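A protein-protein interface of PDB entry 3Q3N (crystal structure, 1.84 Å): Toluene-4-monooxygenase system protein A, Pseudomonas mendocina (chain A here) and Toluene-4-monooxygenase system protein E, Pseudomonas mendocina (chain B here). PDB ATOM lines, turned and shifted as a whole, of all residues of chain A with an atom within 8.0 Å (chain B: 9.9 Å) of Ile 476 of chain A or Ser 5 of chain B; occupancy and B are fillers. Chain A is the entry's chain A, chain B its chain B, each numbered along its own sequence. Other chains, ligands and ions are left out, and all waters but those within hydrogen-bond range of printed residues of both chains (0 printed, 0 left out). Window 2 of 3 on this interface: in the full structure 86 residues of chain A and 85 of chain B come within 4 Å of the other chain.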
ATOM      1  N   ARG A 153       1.133 -18.758 -18.346  1.00  0.00           N
ATOM      2  CA  ARG A 153       0.084 -17.806 -17.996  1.00  0.00           C
ATOM      3  C   ARG A 153      -0.061 -16.670 -19.020  1.00  0.00           C
ATOM      4  O   ARG A 153      -1.108 -16.019 -19.101  1.00  0.00           O
ATOM      5  CB  ARG A 153       0.328 -17.230 -16.595  1.00  0.00           C
ATOM      6  CG  ARG A 153       0.167 -18.262 -15.474  1.00  0.00           C
ATOM      7  CD  ARG A 153       0.312 -17.596 -14.099  1.00  0.00           C
ATOM      8  NE  ARG A 153      -0.699 -16.563 -13.896  1.00  0.00           N
ATOM      9  CZ  ARG A 153      -1.820 -16.734 -13.198  1.00  0.00           C
ATOM     10  NH1 ARG A 153      -2.072 -17.895 -12.608  1.00  0.00           N
ATOM     11  NH2 ARG A 153      -2.685 -15.737 -13.071  1.00  0.00           N
ATOM     12  N   GLN A 154       0.984 -16.417 -19.796  1.00  0.00           N
ATOM     13  CA  GLN A 154       0.875 -15.383 -20.822  1.00  0.00           C
ATOM     14  C   GLN A 154      -0.182 -15.730 -21.868  1.00  0.00           C
ATOM     15  O   GLN A 154      -0.748 -14.839 -22.512  1.00  0.00           O
ATOM     16  CB  GLN A 154       2.228 -15.098 -21.471  1.00  0.00           C
ATOM     17  CG  GLN A 154       3.071 -14.171 -20.630  1.00  0.00           C
ATOM     18  CD  GLN A 154       4.420 -13.846 -21.234  1.00  0.00           C
ATOM     19  OE1 GLN A 154       4.894 -14.537 -22.128  1.00  0.00           O
ATOM     20  NE2 GLN A 154       5.053 -12.778 -20.736  1.00  0.00           N
ATOM     21  N   THR A 340       8.523  -5.214 -20.007  1.00  0.00           N
ATOM     22  CA  THR A 340       7.879  -5.689 -18.780  1.00  0.00           C
ATOM     23  C   THR A 340       6.385  -5.332 -18.726  1.00  0.00           C
ATOM     24  O   THR A 340       5.625  -5.918 -17.966  1.00  0.00           O
ATOM     25  CB  THR A 340       8.619  -5.175 -17.526  1.00  0.00           C
ATOM     26  OG1 THR A 340       8.103  -5.827 -16.359  1.00  0.00           O
ATOM     27  CG2 THR A 340       8.474  -3.662 -17.395  1.00  0.00           C
ATOM     28  N   ALA A 342       4.474  -5.664 -21.439  1.00  0.00           N
ATOM     29  CA  ALA A 342       3.809  -6.469 -22.474  1.00  0.00           C
ATOM     30  C   ALA A 342       3.421  -7.832 -21.909  1.00  0.00           C
ATOM     31  O   ALA A 342       3.941  -8.241 -20.876  1.00  0.00           O
ATOM     32  CB  ALA A 342       4.710  -6.640 -23.701  1.00  0.00           C
ATOM     33  N   ASN A 345       6.937 -11.986 -24.657  1.00  0.00           N
ATOM     34  CA  ASN A 345       8.350 -11.783 -24.386  1.00  0.00           C
ATOM     35  C   ASN A 345       9.082 -11.342 -25.660  1.00  0.00           C
ATOM     36  O   ASN A 345       9.441 -12.171 -26.486  1.00  0.00           O
ATOM     37  CB  ASN A 345       8.954 -13.084 -23.835  1.00  0.00           C
ATOM     38  CG  ASN A 345       8.315 -13.527 -22.514  1.00  0.00           C
ATOM     39  OD1 ASN A 345       7.947 -12.707 -21.672  1.00  0.00           O
ATOM     40  ND2 ASN A 345       8.205 -14.838 -22.322  1.00  0.00           N
ATOM     41  N   PHE A 473      -1.695  -7.023 -14.889  1.00  0.00           N
ATOM     42  CA  PHE A 473      -0.799  -8.150 -14.651  1.00  0.00           C
ATOM     43  C   PHE A 473      -1.084  -8.765 -13.289  1.00  0.00           C
ATOM     44  O   PHE A 473      -1.182  -8.055 -12.295  1.00  0.00           O
ATOM     45  CB  PHE A 473       0.662  -7.737 -14.799  1.00  0.00           C
ATOM     46  CG  PHE A 473       1.035  -7.399 -16.207  1.00  0.00           C
ATOM     47  CD1 PHE A 473       1.314  -8.407 -17.116  1.00  0.00           C
ATOM     48  CD2 PHE A 473       1.063  -6.083 -16.634  1.00  0.00           C
ATOM     49  CE1 PHE A 473       1.638  -8.108 -18.429  1.00  0.00           C
ATOM     50  CE2 PHE A 473       1.384  -5.773 -17.946  1.00  0.00           C
ATOM     51  CZ  PHE A 473       1.678  -6.778 -18.841  1.00  0.00           C
ATOM     52  N   GLN A 474      -1.247 -10.087 -13.267  1.00  0.00           N
ATOM     53  CA  GLN A 474      -1.621 -10.800 -12.045  1.00  0.00           C
ATOM     54  C   GLN A 474      -0.501 -11.649 -11.463  1.00  0.00           C
ATOM     55  O   GLN A 474      -0.675 -12.250 -10.406  1.00  0.00           O
ATOM     56  CB  GLN A 474      -2.857 -11.671 -12.279  1.00  0.00           C
ATOM     57  CG  GLN A 474      -4.140 -10.882 -12.458  1.00  0.00           C
ATOM     58  CD  GLN A 474      -5.285 -11.742 -12.943  1.00  0.00           C
ATOM     59  OE1 GLN A 474      -5.259 -12.965 -12.801  1.00  0.00           O
ATOM     60  NE2 GLN A 474      -6.298 -11.109 -13.529  1.00  0.00           N
ATOM     61  N   SER A 475       0.641 -11.710 -12.141  1.00  0.00           N
ATOM     62  CA  SER A 475       1.802 -12.374 -11.557  1.00  0.00           C
ATOM     63  C   SER A 475       3.084 -12.006 -12.268  1.00  0.00           C
ATOM     64  O   SER A 475       3.076 -11.507 -13.390  1.00  0.00           O
ATOM     65  CB  SER A 475       1.638 -13.900 -11.574  1.00  0.00           C
ATOM     66  OG  SER A 475       1.999 -14.450 -12.834  1.00  0.00           O
ATOM     67  N   ILE A 476       4.194 -12.273 -11.598  1.00  0.00           N
ATOM     68  CA  ILE A 476       5.510 -12.043 -12.169  1.00  0.00           C
ATOM     69  C   ILE A 476       5.640 -12.689 -13.548  1.00  0.00           C
ATOM     70  O   ILE A 476       6.161 -12.076 -14.466  1.00  0.00           O
ATOM     71  CB  ILE A 476       6.618 -12.588 -11.237  1.00  0.00           C
ATOM     72  CG1 ILE A 476       6.603 -11.846  -9.897  1.00  0.00           C
ATOM     73  CG2 ILE A 476       7.986 -12.473 -11.896  1.00  0.00           C
ATOM     74  CD1 ILE A 476       5.441 -12.214  -8.995  1.00  0.00           C
ATOM     75  N   GLU A 477       5.166 -13.925 -13.688  1.00  0.00           N
ATOM     76  CA  GLU A 477       5.352 -14.680 -14.933  1.00  0.00           C
ATOM     77  C   GLU A 477       4.699 -14.069 -16.159  1.00  0.00           C
ATOM     78  O   GLU A 477       5.143 -14.314 -17.280  1.00  0.00           O
ATOM     79  CB  GLU A 477       4.851 -16.116 -14.789  1.00  0.00           C
ATOM     80  CG  GLU A 477       5.628 -16.941 -13.792  1.00  0.00           C
ATOM     81  CD  GLU A 477       5.165 -16.710 -12.372  1.00  0.00           C
ATOM     82  OE1 GLU A 477       3.961 -16.415 -12.180  1.00  0.00           O
ATOM     83  OE2 GLU A 477       6.006 -16.827 -11.455  1.00  0.00           O
ATOM     84  N   GLU A 478       3.637 -13.299 -15.948  1.00  0.00           N
ATOM     85  CA  GLU A 478       2.861 -12.742 -17.054  1.00  0.00           C
ATOM     86  C   GLU A 478       3.557 -11.549 -17.704  1.00  0.00           C
ATOM     87  O   GLU A 478       3.265 -11.207 -18.838  1.00  0.00           O
ATOM     88  CB  GLU A 478       1.459 -12.342 -16.577  1.00  0.00           C
ATOM     89  CG  GLU A 478       0.689 -13.457 -15.882  1.00  0.00           C
ATOM     90  CD  GLU A 478      -0.645 -12.997 -15.327  1.00  0.00           C
ATOM     91  OE1 GLU A 478      -0.955 -11.799 -15.461  1.00  0.00           O
ATOM     92  OE2 GLU A 478      -1.382 -13.831 -14.747  1.00  0.00           O
ATOM     93  N   MET A 479       4.475 -10.911 -16.984  1.00  0.00           N
ATOM     94  CA  MET A 479       5.136  -9.726 -17.522  1.00  0.00           C
ATOM     95  C   MET A 479       6.231 -10.106 -18.509  1.00  0.00           C
ATOM     96  O   MET A 479       6.932 -11.099 -18.312  1.00  0.00           O
ATOM     97  CB  MET A 479       5.712  -8.884 -16.387  1.00  0.00           C
ATOM     98  CG  MET A 479       4.783  -8.776 -15.195  1.00  0.00           C
ATOM     99  SD  MET A 479       5.537  -7.805 -13.888  1.00  0.00           S
ATOM    100  CE  MET A 479       4.378  -8.096 -12.561  1.00  0.00           C
ATOM    101  N   GLY A 480       6.375  -9.310 -19.563  1.00  0.00           N
ATOM    102  CA  GLY A 480       7.333  -9.599 -20.619  1.00  0.00           C
ATOM    103  C   GLY A 480       8.792  -9.537 -20.196  1.00  0.00           C
ATOM    104  O   GLY A 480       9.182  -8.706 -19.373  1.00  0.00           O
ATOM    105  N   LYS A 481       9.598 -10.424 -20.774  1.00  0.00           N
ATOM    106  CA  LYS A 481      11.039 -10.448 -20.538  1.00  0.00           C
ATOM    107  C   LYS A 481      11.704 -10.619 -21.896  1.00  0.00           C
ATOM    108  O   LYS A 481      11.024 -10.905 -22.873  1.00  0.00           O
ATOM    109  CB  LYS A 481      11.401 -11.640 -19.650  1.00  0.00           C
ATOM    110  CG  LYS A 481      10.453 -11.862 -18.480  1.00  0.00           C
ATOM    111  CD  LYS A 481      10.576 -13.286 -17.950  1.00  0.00           C
ATOM    112  CE  LYS A 481       9.218 -13.878 -17.573  1.00  0.00           C
ATOM    113  NZ  LYS A 481       8.226 -13.838 -18.696  1.00  0.00           N
ATOM    114  N   SER B   2       4.129  -6.259  -3.472  1.00  0.00           N
ATOM    115  CA  SER B   2       4.470  -6.818  -4.775  1.00  0.00           C
ATOM    116  C   SER B   2       3.369  -7.739  -5.292  1.00  0.00           C
ATOM    117  O   SER B   2       2.320  -7.884  -4.664  1.00  0.00           O
ATOM    118  CB  SER B   2       5.804  -7.567  -4.709  1.00  0.00           C
ATOM    119  OG  SER B   2       6.184  -8.057  -5.985  1.00  0.00           O
ATOM    120  N   PHE B   3       3.610  -8.347  -6.449  1.00  0.00           N
ATOM    121  CA  PHE B   3       2.706  -9.345  -6.995  1.00  0.00           C
ATOM    122  C   PHE B   3       2.969 -10.669  -6.301  1.00  0.00           C
ATOM    123  O   PHE B   3       3.931 -10.797  -5.545  1.00  0.00           O
ATOM    124  CB  PHE B   3       2.943  -9.513  -8.495  1.00  0.00           C
ATOM    125  CG  PHE B   3       2.785  -8.245  -9.278  1.00  0.00           C
ATOM    126  CD1 PHE B   3       1.631  -8.005 -10.006  1.00  0.00           C
ATOM    127  CD2 PHE B   3       3.788  -7.290  -9.283  1.00  0.00           C
ATOM    128  CE1 PHE B   3       1.481  -6.837 -10.727  1.00  0.00           C
ATOM    129  CE2 PHE B   3       3.644  -6.119 -10.000  1.00  0.00           C
ATOM    130  CZ  PHE B   3       2.489  -5.893 -10.724  1.00  0.00           C
ATOM    131  N   GLU B   4       2.108 -11.647  -6.551  1.00  0.00           N
ATOM    132  CA  GLU B   4       2.368 -13.014  -6.130  1.00  0.00           C
ATOM    133  C   GLU B   4       2.844 -13.809  -7.331  1.00  0.00           C
ATOM    134  O   GLU B   4       2.572 -13.439  -8.472  1.00  0.00           O
ATOM    135  CB  GLU B   4       1.104 -13.666  -5.565  1.00  0.00           C
ATOM    136  CG  GLU B   4       0.626 -13.090  -4.246  1.00  0.00           C
ATOM    137  CD  GLU B   4      -0.805 -12.592  -4.319  1.00  0.00           C
ATOM    138  OE1 GLU B   4      -1.333 -12.460  -5.447  1.00  0.00           O
ATOM    139  OE2 GLU B   4      -1.401 -12.335  -3.250  1.00  0.00           O
ATOM    140  N   SER B   5       3.569 -14.892  -7.072  1.00  0.00           N
ATOM    141  CA  SER B   5       3.962 -15.814  -8.126  1.00  0.00           C
ATOM    142  C   SER B   5       2.888 -16.882  -8.220  1.00  0.00           C
ATOM    143  O   SER B   5       2.503 -17.472  -7.209  1.00  0.00           O
ATOM    144  CB  SER B   5       5.312 -16.457  -7.811  1.00  0.00           C
ATOM    145  OG  SER B   5       6.317 -15.484  -7.587  1.00  0.00           O
ATOM    146  N   LYS B   6       2.397 -17.128  -9.429  1.00  0.00           N
ATOM    147  CA  LYS B   6       1.335 -18.094  -9.619  1.00  0.00           C
ATOM    148  C   LYS B   6       1.674 -19.092 -10.717  1.00  0.00           C
ATOM    149  O   LYS B   6       2.454 -18.804 -11.618  1.00  0.00           O
ATOM    150  CB  LYS B   6       0.027 -17.380  -9.955  1.00  0.00           C
ATOM    151  CG  LYS B   6      -0.411 -16.361  -8.914  1.00  0.00           C
ATOM    152  CD  LYS B   6      -1.687 -15.668  -9.340  1.00  0.00           C
ATOM    153  CE  LYS B   6      -2.220 -14.775  -8.236  1.00  0.00           C
ATOM    154  NZ  LYS B   6      -3.355 -13.939  -8.719  1.00  0.00           N
ATOM    155  N   LYS B   7       1.085 -20.271 -10.632  1.00  0.00           N
ATOM    156  CA  LYS B   7       1.337 -21.282 -11.642  1.00  0.00           C
ATOM    157  C   LYS B   7       0.303 -21.181 -12.750  1.00  0.00           C
ATOM    158  O   LYS B   7      -0.705 -20.492 -12.597  1.00  0.00           O
ATOM    159  CB  LYS B   7       1.353 -22.677 -11.026  1.00  0.00           C
ATOM    160  CG  LYS B   7       0.231 -22.955 -10.063  1.00  0.00           C
ATOM    161  CD  LYS B   7       0.646 -24.059  -9.103  1.00  0.00           C
ATOM    162  CE  LYS B   7      -0.478 -24.434  -8.158  1.00  0.00           C
ATOM    163  NZ  LYS B   7      -0.920 -23.254  -7.368  1.00  0.00           N
ATOM    164  N   PRO B   8       0.563 -21.851 -13.877  1.00  0.00           N
ATOM    165  CA  PRO B   8      -0.390 -21.867 -14.990  1.00  0.00           C
ATOM    166  C   PRO B   8      -1.757 -22.377 -14.540  1.00  0.00           C
ATOM    167  O   PRO B   8      -1.850 -23.199 -13.626  1.00  0.00           O
ATOM    168  CB  PRO B   8       0.241 -22.859 -15.969  1.00  0.00           C
ATOM    169  CG  PRO B   8       1.708 -22.769 -15.698  1.00  0.00           C
ATOM    170  CD  PRO B   8       1.809 -22.570 -14.201  1.00  0.00           C
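The side-chain hydroxyl (OG) of Ser 475 of chain A lies within hydrogen-bond range of the side-chain carboxylate (OE1) of Glu 477 of chain A. NE2 of Gln 154 of chain A sits at hydrogen-bond distance from O of Met 479 of chain A, 3.5 Å away. The side-chain carboxylate of Glu 478 of chain A is in salt-bridge range of the guanidinium group of Arg 153 of chain A (2.9 Å). NZ of Lys 481 of chain A is in hydrogen-bond range of O of Glu 477 of chain A. The side-chain amino group (NZ) of Lys 481 of chain A sits at hydrogen-bond distance from the backbone carbonyl oxygen (O) of Met 479 of chain A. The side-chain carboxylate (OE1) of Glu 478 of chain A is in hydrogen-bond range of the backbone NH (N) of Gln 474 of chain A (2.8 Å).
The backbone NH of Lys 6 of chain B is in hydrogen-bond range of the side-chain carboxylate of Glu 477 of chain A, at 3.2 Å. The backbone carbonyl oxygen (O) of Lys 7 of chain B sits at hydrogen-bond distance from the guanidinium group (NH1) of Arg 153 of chain A (2.9 Å).
Among the printed residues, pairs that only touch across the chains: Ile 476 of chain A with Glu 4 of chain B, Ser 475 of chain A with Glu 4 of chain B, Met 479 of chain A with Phe 3 of chain B, Phe 473 of chain A with Phe 3 of chain B, Arg 153 of chain A with Lys 6 of chain B, Gln 474 of chain A with Lys 6 of chain B, Ile 476 of chain A with Ser 5 of chain B, Arg 153 of chain A with Pro 8 of chain B, Ile 476 of chain A with Phe 3 of chain B, Glu 477 of chain A with Ser 5 of chain B, Ser 475 of chain A with Lys 6 of chain B and Gln 474 of chain A with Glu 4 of chain B.
Of the printed residues of chain B, Arg 153 of chain A touches Lys 6, Lys 7 and Pro 8. Thr 340 of chain A touches none of the printed residues of chain B. Of the printed residues of chain B, Gln 474 of chain A touches Glu 4 and Lys 6. Ser 475 of chain A touches two residues of chain B. Printed residues of chain B within 4 Å of Ile 476 of chain A: Phe 3 (3.7 Å), Glu 4 (3.2 Å) and Ser 5 (3.7 Å). Glu 478 of chain A touches none of the printed residues of chain B. Of the printed residues of chain A, Ser 5 of chain B touches Ile 476 (3.7 Å) and Glu 477 (3.7 Å). Of the printed residues of chain A, Lys 6 of chain B touches Arg 153 (3.4 Å), Gln 474 (3.6 Å), Ser 475 (3.9 Å) and Glu 477 (2.9 Å). Printed residues of chain A within 4 Å of Pro 8 of chain B: Arg 153 (3.7 Å). The nearest printed residue of chain B that does not touch Ile 476 of chain A is Ser 2 of chain B (5.2 Å). The nearest printed residue of chain A that does not touch Ser 5 of chain B is Ser 475 of chain A (4.6 Å).
Hydrophobic or aromatic side chains of chain A within 4 Å of the printed part of chain B: Ile 476 and Met 479. Of the 7 printed residues of chain B, 6 touch a printed residue of chain A. Printed residues of chain B that touch a printed residue of chain A: Phe 3, Glu 4, Ser 5, Lys 6, Lys 7 and Pro 8. Hydrophobic or aromatic side chains of chain B that line the printed part of chain A: Phe 3. Among the printed residues, no Asp or Glu carboxylate lies within 4 Å of a Lys or Arg side-chain nitrogen of the other chain.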
